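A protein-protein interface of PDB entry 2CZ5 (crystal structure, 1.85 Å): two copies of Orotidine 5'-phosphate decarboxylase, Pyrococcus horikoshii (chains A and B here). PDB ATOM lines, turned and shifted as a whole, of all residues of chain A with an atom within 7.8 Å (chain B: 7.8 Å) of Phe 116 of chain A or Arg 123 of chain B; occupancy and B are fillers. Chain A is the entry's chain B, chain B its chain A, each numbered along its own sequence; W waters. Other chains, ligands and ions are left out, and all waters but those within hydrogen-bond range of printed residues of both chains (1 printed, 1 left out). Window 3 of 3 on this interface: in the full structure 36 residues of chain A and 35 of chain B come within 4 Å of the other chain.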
ATOM      1  N   PHE A  87      29.891   3.177   1.615  1.00  0.00           N
ATOM      2  CA  PHE A  87      28.665   2.589   1.077  1.00  0.00           C
ATOM      3  C   PHE A  87      27.395   3.438   1.008  1.00  0.00           C
ATOM      4  O   PHE A  87      26.490   3.120   0.230  1.00  0.00           O
ATOM      5  CB  PHE A  87      28.373   1.257   1.777  1.00  0.00           C
ATOM      6  CG  PHE A  87      27.759   1.377   3.139  1.00  0.00           C
ATOM      7  CD1 PHE A  87      26.394   1.613   3.283  1.00  0.00           C
ATOM      8  CD2 PHE A  87      28.518   1.125   4.277  1.00  0.00           C
ATOM      9  CE1 PHE A  87      25.784   1.577   4.544  1.00  0.00           C
ATOM     10  CE2 PHE A  87      27.920   1.090   5.549  1.00  0.00           C
ATOM     11  CZ  PHE A  87      26.544   1.313   5.676  1.00  0.00           C
ATOM     12  N   PRO A 111      33.418 -11.149  10.497  1.00  0.00           N
ATOM     13  CA  PRO A 111      32.802 -12.106   9.571  1.00  0.00           C
ATOM     14  C   PRO A 111      31.702 -11.507   8.691  1.00  0.00           C
ATOM     15  O   PRO A 111      31.592 -11.834   7.515  1.00  0.00           O
ATOM     16  CB  PRO A 111      32.283 -13.205  10.505  1.00  0.00           C
ATOM     17  CG  PRO A 111      33.243 -13.180  11.636  1.00  0.00           C
ATOM     18  CD  PRO A 111      33.450 -11.679  11.872  1.00  0.00           C
ATOM     19  N   GLY A 112      30.901 -10.615   9.261  1.00  0.00           N
ATOM     20  CA  GLY A 112      29.824  -9.990   8.507  1.00  0.00           C
ATOM     21  C   GLY A 112      30.274  -9.136   7.335  1.00  0.00           C
ATOM     22  O   GLY A 112      29.507  -8.873   6.417  1.00  0.00           O
ATOM     23  N   ALA A 113      31.529  -8.701   7.345  1.00  0.00           N
ATOM     24  CA  ALA A 113      32.025  -7.879   6.245  1.00  0.00           C
ATOM     25  C   ALA A 113      32.051  -8.683   4.947  1.00  0.00           C
ATOM     26  O   ALA A 113      32.000  -8.124   3.853  1.00  0.00           O
ATOM     27  CB  ALA A 113      33.421  -7.380   6.559  1.00  0.00           C
ATOM     28  N   LEU A 114      32.140 -10.004   5.052  1.00  0.00           N
ATOM     29  CA  LEU A 114      32.182 -10.815   3.839  1.00  0.00           C
ATOM     30  C   LEU A 114      30.876 -10.772   3.060  1.00  0.00           C
ATOM     31  O   LEU A 114      30.846 -11.108   1.878  1.00  0.00           O
ATOM     32  CB  LEU A 114      32.504 -12.281   4.166  1.00  0.00           C
ATOM     33  CG  LEU A 114      33.903 -12.631   4.685  1.00  0.00           C
ATOM     34  CD1 LEU A 114      34.963 -12.254   3.666  1.00  0.00           C
ATOM     35  CD2 LEU A 114      34.152 -11.912   5.995  1.00  0.00           C
ATOM     36  N   GLU A 115      29.807 -10.348   3.718  1.00  0.00           N
ATOM     37  CA  GLU A 115      28.497 -10.324   3.095  1.00  0.00           C
ATOM     38  C   GLU A 115      28.196  -9.222   2.089  1.00  0.00           C
ATOM     39  O   GLU A 115      27.623  -9.512   1.037  1.00  0.00           O
ATOM     40  CB  GLU A 115      27.413 -10.365   4.186  1.00  0.00           C
ATOM     41  CG  GLU A 115      27.323 -11.727   4.893  1.00  0.00           C
ATOM     42  CD  GLU A 115      26.649 -11.664   6.258  1.00  0.00           C
ATOM     43  OE1 GLU A 115      25.820 -10.766   6.484  1.00  0.00           O
ATOM     44  OE2 GLU A 115      26.938 -12.527   7.111  1.00  0.00           O
ATOM     45  N   PHE A 116      28.593  -7.974   2.376  1.00  0.00           N
ATOM     46  CA  PHE A 116      28.296  -6.879   1.449  1.00  0.00           C
ATOM     47  C   PHE A 116      29.412  -5.871   1.285  1.00  0.00           C
ATOM     48  O   PHE A 116      29.619  -5.338   0.199  1.00  0.00           O
ATOM     49  CB  PHE A 116      27.050  -6.104   1.901  1.00  0.00           C
ATOM     50  CG  PHE A 116      25.844  -6.962   2.082  1.00  0.00           C
ATOM     51  CD1 PHE A 116      25.405  -7.303   3.353  1.00  0.00           C
ATOM     52  CD2 PHE A 116      25.183  -7.476   0.979  1.00  0.00           C
ATOM     53  CE1 PHE A 116      24.317  -8.159   3.529  1.00  0.00           C
ATOM     54  CE2 PHE A 116      24.089  -8.340   1.146  1.00  0.00           C
ATOM     55  CZ  PHE A 116      23.666  -8.675   2.417  1.00  0.00           C
ATOM     56  N   ILE A 117      30.120  -5.604   2.370  1.00  0.00           N
ATOM     57  CA  ILE A 117      31.199  -4.620   2.348  1.00  0.00           C
ATOM     58  C   ILE A 117      32.408  -5.061   1.539  1.00  0.00           C
ATOM     59  O   ILE A 117      32.773  -4.429   0.562  1.00  0.00           O
ATOM     60  CB  ILE A 117      31.688  -4.301   3.778  1.00  0.00           C
ATOM     61  CG1 ILE A 117      30.590  -3.583   4.577  1.00  0.00           C
ATOM     62  CG2 ILE A 117      32.977  -3.489   3.711  1.00  0.00           C
ATOM     63  CD1 ILE A 117      30.430  -2.080   4.279  1.00  0.00           C
ATOM     64  N   ASN A 118      33.024  -6.164   1.940  1.00  0.00           N
ATOM     65  CA  ASN A 118      34.227  -6.606   1.259  1.00  0.00           C
ATOM     66  C   ASN A 118      34.081  -6.944  -0.235  1.00  0.00           C
ATOM     67  O   ASN A 118      35.016  -6.721  -1.014  1.00  0.00           O
ATOM     68  CB  ASN A 118      34.885  -7.717   2.084  1.00  0.00           C
ATOM     69  CG  ASN A 118      35.416  -7.188   3.418  1.00  0.00           C
ATOM     70  OD1 ASN A 118      35.159  -6.039   3.782  1.00  0.00           O
ATOM     71  ND2 ASN A 118      36.152  -8.016   4.148  1.00  0.00           N
ATOM     72  N   PRO A 119      32.920  -7.475  -0.659  1.00  0.00           N
ATOM     73  CA  PRO A 119      32.825  -7.756  -2.095  1.00  0.00           C
ATOM     74  C   PRO A 119      32.901  -6.438  -2.898  1.00  0.00           C
ATOM     75  O   PRO A 119      33.093  -6.449  -4.121  1.00  0.00           O
ATOM     76  CB  PRO A 119      31.459  -8.429  -2.221  1.00  0.00           C
ATOM     77  CG  PRO A 119      31.386  -9.212  -0.965  1.00  0.00           C
ATOM     78  CD  PRO A 119      31.907  -8.246   0.088  1.00  0.00           C
ATOM     79  N   LEU A 120      32.775  -5.311  -2.194  1.00  0.00           N
ATOM     80  CA  LEU A 120      32.795  -3.990  -2.823  1.00  0.00           C
ATOM     81  C   LEU A 120      34.050  -3.161  -2.577  1.00  0.00           C
ATOM     82  O   LEU A 120      34.114  -2.007  -2.996  1.00  0.00           O
ATOM     83  CB  LEU A 120      31.570  -3.164  -2.375  1.00  0.00           C
ATOM     84  CG  LEU A 120      30.185  -3.500  -2.947  1.00  0.00           C
ATOM     85  CD1 LEU A 120      29.095  -2.745  -2.196  1.00  0.00           C
ATOM     86  CD2 LEU A 120      30.157  -3.164  -4.434  1.00  0.00           C
ATOM     87  N   THR A 121      35.046  -3.731  -1.911  1.00  0.00           N
ATOM     88  CA  THR A 121      36.283  -2.997  -1.624  1.00  0.00           C
ATOM     89  C   THR A 121      36.939  -2.407  -2.874  1.00  0.00           C
ATOM     90  O   THR A 121      37.372  -1.248  -2.867  1.00  0.00           O
ATOM     91  CB  THR A 121      37.296  -3.899  -0.874  1.00  0.00           C
ATOM     92  OG1 THR A 121      36.766  -4.211   0.422  1.00  0.00           O
ATOM     93  CG2 THR A 121      38.651  -3.200  -0.716  1.00  0.00           C
ATOM     94  N   PHE A 124      35.006   0.506  -3.789  1.00  0.00           N
ATOM     95  CA  PHE A 124      35.096   1.593  -2.817  1.00  0.00           C
ATOM     96  C   PHE A 124      36.416   2.334  -2.996  1.00  0.00           C
ATOM     97  O   PHE A 124      36.475   3.534  -2.773  1.00  0.00           O
ATOM     98  CB  PHE A 124      34.997   1.094  -1.365  1.00  0.00           C
ATOM     99  CG  PHE A 124      33.645   0.559  -0.986  1.00  0.00           C
ATOM    100  CD1 PHE A 124      32.482   1.042  -1.592  1.00  0.00           C
ATOM    101  CD2 PHE A 124      33.532  -0.410   0.001  1.00  0.00           C
ATOM    102  CE1 PHE A 124      31.229   0.563  -1.215  1.00  0.00           C
ATOM    103  CE2 PHE A 124      32.279  -0.900   0.390  1.00  0.00           C
ATOM    104  CZ  PHE A 124      31.126  -0.409  -0.220  1.00  0.00           C
ATOM    105  N   THR B  86      21.861  -2.655   7.483  1.00  0.00           N
ATOM    106  CA  THR B  86      21.913  -4.081   7.153  1.00  0.00           C
ATOM    107  C   THR B  86      23.238  -4.385   6.440  1.00  0.00           C
ATOM    108  O   THR B  86      23.777  -5.486   6.542  1.00  0.00           O
ATOM    109  CB  THR B  86      20.762  -4.479   6.206  1.00  0.00           C
ATOM    110  OG1 THR B  86      19.509  -4.061   6.768  1.00  0.00           O
ATOM    111  CG2 THR B  86      20.747  -5.974   5.992  1.00  0.00           C
ATOM    112  N   PHE B  87      23.766  -3.367   5.758  1.00  0.00           N
ATOM    113  CA  PHE B  87      24.988  -3.439   4.961  1.00  0.00           C
ATOM    114  C   PHE B  87      26.242  -4.026   5.618  1.00  0.00           C
ATOM    115  O   PHE B  87      27.021  -4.718   4.965  1.00  0.00           O
ATOM    116  CB  PHE B  87      25.317  -2.038   4.451  1.00  0.00           C
ATOM    117  CG  PHE B  87      25.866  -2.010   3.064  1.00  0.00           C
ATOM    118  CD1 PHE B  87      27.073  -2.646   2.755  1.00  0.00           C
ATOM    119  CD2 PHE B  87      25.181  -1.350   2.059  1.00  0.00           C
ATOM    120  CE1 PHE B  87      27.582  -2.624   1.453  1.00  0.00           C
ATOM    121  CE2 PHE B  87      25.686  -1.324   0.750  1.00  0.00           C
ATOM    122  CZ  PHE B  87      26.884  -1.964   0.454  1.00  0.00           C
ATOM    123  N   VAL B  88      26.430  -3.777   6.906  1.00  0.00           N
ATOM    124  CA  VAL B  88      27.627  -4.266   7.577  1.00  0.00           C
ATOM    125  C   VAL B  88      27.587  -5.752   7.967  1.00  0.00           C
ATOM    126  O   VAL B  88      28.561  -6.299   8.481  1.00  0.00           O
ATOM    127  CB  VAL B  88      27.942  -3.356   8.780  1.00  0.00           C
ATOM    128  CG1 VAL B  88      29.136  -3.865   9.567  1.00  0.00           C
ATOM    129  CG2 VAL B  88      28.265  -1.956   8.245  1.00  0.00           C
ATOM    130  N   GLY B  89      26.460  -6.407   7.721  1.00  0.00           N
ATOM    131  CA  GLY B  89      26.413  -7.833   8.015  1.00  0.00           C
ATOM    132  C   GLY B  89      25.485  -8.290   9.113  1.00  0.00           C
ATOM    133  O   GLY B  89      25.154  -7.545  10.027  1.00  0.00           O
ATOM    134  N   ARG B  90      25.094  -9.560   9.040  1.00  0.00           N
ATOM    135  CA  ARG B  90      24.183 -10.100  10.032  1.00  0.00           C
ATOM    136  C   ARG B  90      24.724 -10.102  11.455  1.00  0.00           C
ATOM    137  O   ARG B  90      23.993  -9.773  12.399  1.00  0.00           O
ATOM    138  CB  ARG B  90      23.777 -11.530   9.652  1.00  0.00           C
ATOM    139  CG  ARG B  90      22.809 -12.135  10.653  1.00  0.00           C
ATOM    140  CD  ARG B  90      22.391 -13.552  10.272  1.00  0.00           C
ATOM    141  NE  ARG B  90      21.418 -14.041  11.241  1.00  0.00           N
ATOM    142  CZ  ARG B  90      21.087 -15.313  11.410  1.00  0.00           C
ATOM    143  NH1 ARG B  90      21.647 -16.264  10.662  1.00  0.00           N
ATOM    144  NH2 ARG B  90      20.203 -15.634  12.347  1.00  0.00           N
ATOM    145  N   MET B 104      15.846  -1.934  10.925  1.00  0.00           N
ATOM    146  CA  MET B 104      16.893  -2.099   9.924  1.00  0.00           C
ATOM    147  C   MET B 104      16.765  -1.213   8.690  1.00  0.00           C
ATOM    148  O   MET B 104      15.685  -1.027   8.141  1.00  0.00           O
ATOM    149  CB  MET B 104      16.945  -3.574   9.500  1.00  0.00           C
ATOM    150  CG  MET B 104      17.519  -4.502  10.559  1.00  0.00           C
ATOM    151  SD  MET B 104      17.277  -6.286  10.130  1.00  0.00           S
ATOM    152  CE  MET B 104      18.353  -6.445   8.762  1.00  0.00           C
ATOM    153  N   VAL B 106      16.957  -0.716   4.994  1.00  0.00           N
ATOM    154  CA  VAL B 106      17.011  -1.552   3.812  1.00  0.00           C
ATOM    155  C   VAL B 106      17.069  -0.749   2.529  1.00  0.00           C
ATOM    156  O   VAL B 106      17.433  -1.286   1.488  1.00  0.00           O
ATOM    157  CB  VAL B 106      15.822  -2.547   3.751  1.00  0.00           C
ATOM    158  CG1 VAL B 106      15.836  -3.421   4.978  1.00  0.00           C
ATOM    159  CG2 VAL B 106      14.507  -1.799   3.634  1.00  0.00           C
ATOM    160  N   PHE B 116      25.060   2.094  -3.957  1.00  0.00           N
ATOM    161  CA  PHE B 116      25.296   0.793  -3.344  1.00  0.00           C
ATOM    162  C   PHE B 116      24.152   0.217  -2.544  1.00  0.00           C
ATOM    163  O   PHE B 116      23.878  -0.981  -2.624  1.00  0.00           O
ATOM    164  CB  PHE B 116      26.516   0.853  -2.422  1.00  0.00           C
ATOM    165  CG  PHE B 116      27.768   1.326  -3.102  1.00  0.00           C
ATOM    166  CD1 PHE B 116      28.256   2.612  -2.872  1.00  0.00           C
ATOM    167  CD2 PHE B 116      28.458   0.485  -3.977  1.00  0.00           C
ATOM    168  CE1 PHE B 116      29.416   3.049  -3.505  1.00  0.00           C
ATOM    169  CE2 PHE B 116      29.614   0.908  -4.612  1.00  0.00           C
ATOM    170  CZ  PHE B 116      30.099   2.197  -4.377  1.00  0.00           C
ATOM    171  N   ILE B 117      23.502   1.060  -1.747  1.00  0.00           N
ATOM    172  CA  ILE B 117      22.416   0.594  -0.898  1.00  0.00           C
ATOM    173  C   ILE B 117      21.181   0.065  -1.617  1.00  0.00           C
ATOM    174  O   ILE B 117      20.790  -1.094  -1.432  1.00  0.00           O
ATOM    175  CB  ILE B 117      21.977   1.694   0.076  1.00  0.00           C
ATOM    176  CG1 ILE B 117      23.143   2.043   1.010  1.00  0.00           C
ATOM    177  CG2 ILE B 117      20.765   1.235   0.870  1.00  0.00           C
ATOM    178  CD1 ILE B 117      22.832   3.170   1.989  1.00  0.00           C
ATOM    179  N   ASN B 118      20.570   0.909  -2.438  1.00  0.00           N
ATOM    180  CA  ASN B 118      19.349   0.521  -3.131  1.00  0.00           C
ATOM    181  C   ASN B 118      19.469  -0.715  -4.040  1.00  0.00           C
ATOM    182  O   ASN B 118      18.526  -1.498  -4.143  1.00  0.00           O
ATOM    183  CB  ASN B 118      18.766   1.763  -3.811  1.00  0.00           C
ATOM    184  CG  ASN B 118      18.299   2.795  -2.779  1.00  0.00           C
ATOM    185  OD1 ASN B 118      18.603   2.665  -1.589  1.00  0.00           O
ATOM    186  ND2 ASN B 118      17.568   3.809  -3.219  1.00  0.00           N
ATOM    187  N   PRO B 119      20.624  -0.909  -4.705  1.00  0.00           N
ATOM    188  CA  PRO B 119      20.788  -2.094  -5.556  1.00  0.00           C
ATOM    189  C   PRO B 119      20.656  -3.397  -4.745  1.00  0.00           C
ATOM    190  O   PRO B 119      20.386  -4.455  -5.312  1.00  0.00           O
ATOM    191  CB  PRO B 119      22.201  -1.937  -6.090  1.00  0.00           C
ATOM    192  CG  PRO B 119      22.299  -0.459  -6.291  1.00  0.00           C
ATOM    193  CD  PRO B 119      21.609   0.129  -5.067  1.00  0.00           C
ATOM    194  N   LEU B 120      20.855  -3.310  -3.424  1.00  0.00           N
ATOM    195  CA  LEU B 120      20.794  -4.482  -2.543  1.00  0.00           C
ATOM    196  C   LEU B 120      19.524  -4.582  -1.724  1.00  0.00           C
ATOM    197  O   LEU B 120      19.393  -5.459  -0.878  1.00  0.00           O
ATOM    198  CB  LEU B 120      21.989  -4.491  -1.578  1.00  0.00           C
ATOM    199  CG  LEU B 120      23.363  -4.805  -2.188  1.00  0.00           C
ATOM    200  CD1 LEU B 120      24.497  -4.541  -1.175  1.00  0.00           C
ATOM    201  CD2 LEU B 120      23.380  -6.253  -2.628  1.00  0.00           C
ATOM    202  N   THR B 121      18.581  -3.688  -1.974  1.00  0.00           N
ATOM    203  CA  THR B 121      17.354  -3.694  -1.212  1.00  0.00           C
ATOM    204  C   THR B 121      16.639  -5.051  -1.214  1.00  0.00           C
ATOM    205  O   THR B 121      16.209  -5.503  -0.164  1.00  0.00           O
ATOM    206  CB  THR B 121      16.406  -2.582  -1.701  1.00  0.00           C
ATOM    207  OG1 THR B 121      17.026  -1.302  -1.465  1.00  0.00           O
ATOM    208  CG2 THR B 121      15.086  -2.635  -0.944  1.00  0.00           C
ATOM    209  N   ASP B 122      16.525  -5.706  -2.363  1.00  0.00           N
ATOM    210  CA  ASP B 122      15.826  -7.003  -2.371  1.00  0.00           C
ATOM    211  C   ASP B 122      16.527  -7.970  -1.437  1.00  0.00           C
ATOM    212  O   ASP B 122      15.884  -8.705  -0.695  1.00  0.00           O
ATOM    213  CB  ASP B 122      15.768  -7.616  -3.773  1.00  0.00           C
ATOM    214  CG  ASP B 122      14.888  -6.836  -4.714  1.00  0.00           C
ATOM    215  OD1 ASP B 122      14.127  -5.960  -4.255  1.00  0.00           O
ATOM    216  OD2 ASP B 122      14.954  -7.108  -5.927  1.00  0.00           O
ATOM    217  N   ARG B 123      17.856  -7.966  -1.478  1.00  0.00           N
ATOM    218  CA  ARG B 123      18.627  -8.842  -0.615  1.00  0.00           C
ATOM    219  C   ARG B 123      18.439  -8.427   0.845  1.00  0.00           C
ATOM    220  O   ARG B 123      18.253  -9.280   1.714  1.00  0.00           O
ATOM    221  CB  ARG B 123      20.114  -8.796  -1.005  1.00  0.00           C
ATOM    222  CG  ARG B 123      21.004  -9.693  -0.177  1.00  0.00           C
ATOM    223  CD  ARG B 123      20.740 -11.177  -0.435  1.00  0.00           C
ATOM    224  NE  ARG B 123      21.530 -12.014   0.469  1.00  0.00           N
ATOM    225  CZ  ARG B 123      21.012 -12.784   1.418  1.00  0.00           C
ATOM    226  NH1 ARG B 123      19.692 -12.832   1.591  1.00  0.00           N
ATOM    227  NH2 ARG B 123      21.812 -13.502   2.202  1.00  0.00           N
ATOM    228  N   PHE B 124      18.466  -7.121   1.120  1.00  0.00           N
ATOM    229  CA  PHE B 124      18.293  -6.661   2.497  1.00  0.00           C
ATOM    230  C   PHE B 124      16.921  -6.991   3.068  1.00  0.00           C
ATOM    231  O   PHE B 124      16.783  -7.231   4.266  1.00  0.00           O
ATOM    232  CB  PHE B 124      18.525  -5.149   2.610  1.00  0.00           C
ATOM    233  CG  PHE B 124      19.934  -4.724   2.321  1.00  0.00           C
ATOM    234  CD1 PHE B 124      21.000  -5.621   2.446  1.00  0.00           C
ATOM    235  CD2 PHE B 124      20.206  -3.393   2.000  1.00  0.00           C
ATOM    236  CE1 PHE B 124      22.318  -5.185   2.260  1.00  0.00           C
ATOM    237  CE2 PHE B 124      21.500  -2.950   1.817  1.00  0.00           C
ATOM    238  CZ  PHE B 124      22.567  -3.840   1.946  1.00  0.00           C
ATOM    239  N   ILE B 125      15.901  -6.983   2.223  1.00  0.00           N
ATOM    240  CA  ILE B 125      14.569  -7.310   2.697  1.00  0.00           C
ATOM    241  C   ILE B 125      14.576  -8.767   3.135  1.00  0.00           C
ATOM    242  O   ILE B 125      13.976  -9.119   4.154  1.00  0.00           O
ATOM    243  CB  ILE B 125      13.506  -7.114   1.598  1.00  0.00           C
ATOM    244  CG1 ILE B 125      13.342  -5.622   1.294  1.00  0.00           C
ATOM    245  CG2 ILE B 125      12.188  -7.743   2.037  1.00  0.00           C
ATOM    246  CD1 ILE B 125      12.612  -5.357   0.005  1.00  0.00           C
ATOM    247  N   GLU B 126      15.265  -9.614   2.381  1.00  0.00           N
ATOM    248  CA  GLU B 126      15.333 -11.031   2.745  1.00  0.00           C
ATOM    249  C   GLU B 126      16.130 -11.274   4.034  1.00  0.00           C
ATOM    250  O   GLU B 126      15.850 -12.210   4.784  1.00  0.00           O
ATOM    251  CB  GLU B 126      15.910 -11.853   1.591  1.00  0.00           C
ATOM    252  CG  GLU B 126      15.092 -11.732   0.316  1.00  0.00           C
ATOM    253  CD  GLU B 126      13.604 -12.014   0.540  1.00  0.00           C
ATOM    254  OE1 GLU B 126      12.786 -11.526  -0.268  1.00  0.00           O
ATOM    255  OE2 GLU B 126      13.252 -12.725   1.515  1.00  0.00           O
ATOM    256  N   VAL B 127      17.120 -10.429   4.306  1.00  0.00           N
ATOM    257  CA  VAL B 127      17.897 -10.587   5.529  1.00  0.00           C
ATOM    258  C   VAL B 127      17.037 -10.186   6.714  1.00  0.00           C
ATOM    259  O   VAL B 127      17.024 -10.875   7.740  1.00  0.00           O
ATOM    260  CB  VAL B 127      19.179  -9.715   5.518  1.00  0.00           C
ATOM    261  CG1 VAL B 127      19.958  -9.914   6.811  1.00  0.00           C
ATOM    262  CG2 VAL B 127      20.042 -10.101   4.338  1.00  0.00           C
ATOM    263  N   ALA B 128      16.305  -9.082   6.552  1.00  0.00           N
ATOM    264  CA  ALA B 128      15.422  -8.565   7.592  1.00  0.00           C
ATOM    265  C   ALA B 128      14.337  -9.602   7.889  1.00  0.00           C
ATOM    266  O   ALA B 128      13.974  -9.809   9.045  1.00  0.00           O
ATOM    267  CB  ALA B 128      14.773  -7.258   7.135  1.00  0.00           C
ATOM    268  N   ASN B 129      13.817 -10.237   6.841  1.00  0.00           N
ATOM    269  CA  ASN B 129      12.777 -11.250   7.023  1.00  0.00           C
ATOM    270  C   ASN B 129      13.278 -12.384   7.914  1.00  0.00           C
ATOM    271  O   ASN B 129      12.526 -12.936   8.706  1.00  0.00           O
ATOM    272  CB  ASN B 129      12.321 -11.822   5.672  1.00  0.00           C
ATOM    273  CG  ASN B 129      11.335 -10.907   4.944  1.00  0.00           C
ATOM    274  OD1 ASN B 129      10.719 -10.038   5.551  1.00  0.00           O
ATOM    275  ND2 ASN B 129      11.166 -11.127   3.642  1.00  0.00           N
ATOM    276  N   GLU B 130      14.552 -12.732   7.781  1.00  0.00           N
ATOM    277  CA  GLU B 130      15.124 -13.805   8.583  1.00  0.00           C
ATOM    278  C   GLU B 130      15.356 -13.374  10.039  1.00  0.00           C
ATOM    279  O   GLU B 130      15.043 -14.107  10.991  1.00  0.00           O
ATOM    280  CB  GLU B 130      16.422 -14.270   7.906  1.00  0.00           C
ATOM    281  CG  GLU B 130      17.137 -15.436   8.568  1.00  0.00           C
ATOM    282  CD  GLU B 130      18.142 -14.993   9.619  1.00  0.00           C
ATOM    283  OE1 GLU B 130      18.952 -14.079   9.318  1.00  0.00           O
ATOM    284  OE2 GLU B 130      18.127 -15.570  10.734  1.00  0.00           O
ATOM    285  N   TYR B 148       6.208  -1.807  -2.561  1.00  0.00           N
ATOM    286  CA  TYR B 148       7.121  -2.785  -3.136  1.00  0.00           C
ATOM    287  C   TYR B 148       7.737  -3.568  -1.986  1.00  0.00           C
ATOM    288  O   TYR B 148       7.821  -4.799  -2.009  1.00  0.00           O
ATOM    289  CB  TYR B 148       8.226  -2.069  -3.915  1.00  0.00           C
ATOM    290  CG  TYR B 148       9.271  -2.995  -4.486  1.00  0.00           C
ATOM    291  CD1 TYR B 148       9.185  -3.450  -5.803  1.00  0.00           C
ATOM    292  CD2 TYR B 148      10.335  -3.440  -3.700  1.00  0.00           C
ATOM    293  CE1 TYR B 148      10.139  -4.332  -6.324  1.00  0.00           C
ATOM    294  CE2 TYR B 148      11.292  -4.319  -4.208  1.00  0.00           C
ATOM    295  CZ  TYR B 148      11.187  -4.761  -5.518  1.00  0.00           C
ATOM    296  OH  TYR B 148      12.121  -5.637  -6.012  1.00  0.00           O
HETATM  297  O   HOH W   1      24.434   3.630  -1.648  1.00  0.00           O
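N of Arg 90 of chain B sits at hydrogen-bond distance from OE1 of Glu 115 of chain A (2.9 Å).
The backbone carbonyl oxygen of Gly 112 of chain A sits close to the backbone carbonyl oxygen of Val 88 of chain B, at 3.4 Å.
Phe 87 of chain A touches its own counterpart, Phe 87 of chain B.
Phe 87 of chain A touches Phe 116 of chain B, and with the chains exchanged Phe 116 of chain A touches Phe 87 of chain B.
Phe 116 of chain A touches Leu 120 of chain B, and with the chains exchanged Leu 120 of chain A touches Phe 116 of chain B.
Phe 116 of chain A touches Phe 124 of chain B, and with the chains exchanged Phe 124 of chain A touches Phe 116 of chain B.
Positions printed for both chains: 87, 116, 117, 118, 119, 120, 121 and 124.
Of the 16 pairs that touch across the chains among the printed residues, 9 have their exchanged pair printed and touching as well.
The guanidinium group (NH2) of Arg 90 of chain B is in salt-bridge range of the side-chain carboxylate (OE2) of Glu 130 of chain B, at 2.6 Å.
The backbone carbonyl oxygen (O) of Ala 113 of chain A is in hydrogen-bond range of the backbone NH (N) of Asn 118 of chain A, 2.9 Å away.
Hydrophobic or aromatic side chains of chain A within 4 Å of the printed part of chain B: Phe 87, Phe 116, Ile 117, Leu 120 and Phe 124.
Of the 23 printed residues of chain B, 9 touch a printed residue of chain A.
Among the printed residues, no Asp or Glu carboxylate lies within 4 Å of a Lys or Arg side-chain nitrogen of the other chain.
Printed residues of chain B within 4 Å of Phe 116 of chain A: Phe 87, Leu 120, Arg 123 and Phe 124.
Of the printed residues of chain A, Arg 123 of chain B touches Phe 116 (3.6 Å).
Of the printed residues of chain A, Val 88 of chain B touches Gly 112 (3.4 Å) and Ala 113 (3.98 Å).
Of the printed residues of chain B, Leu 120 of chain A touches Phe 87 (3.5 Å) and Phe 116 (3.7 Å).
Ile 125 of chain B touches none of the printed residues of chain A.
The nearest printed residue of chain B that does not touch Phe 116 of chain A is Thr 86 of chain B (4.02 Å).
The nearest residue of chain A that does not touch Arg 123 of chain B is Glu 115 of chain A (6.4 Å).
The nearest printed residue of chain A that does not touch Phe 87 of chain B is Phe 124 of chain A (4.5 Å).
CD2 of Phe 87 of chain B touches CD1 of Phe 87 of chain A, at 3.4 Å.
Phe 87 of chain A touches Phe 116 of chain B.
Phe 87 of chain A touches Ile 117 of chain B (O to CG1, 3.6 Å).
Ala 113 of chain A touches Val 88 of chain B.
Phe 116 of chain A touches Leu 120 of chain B (CD2 to CD1, 3.7 Å).
Phe 116 of chain A touches Arg 123 of chain B (CE2 to CG, 3.6 Å).
Phe 116 of chain A touches Phe 124 of chain B (CZ to CE1, 3.7 Å).
CD1 of Ile 117 of chain A touches CD1 of Phe 87 of chain B, 3.7 Å away.
Leu 120 of chain A touches Phe 87 of chain B.
Phe 124 of chain A touches Phe 116 of chain B (CE1 to CZ, 3.7 Å).
Water W1 lies within hydrogen-bond range of N of Ile 117 of chain B (2.7 Å), O of Phe 87 of chain A (2.8 Å) and N of Phe 116 of chain B (2.8 Å).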
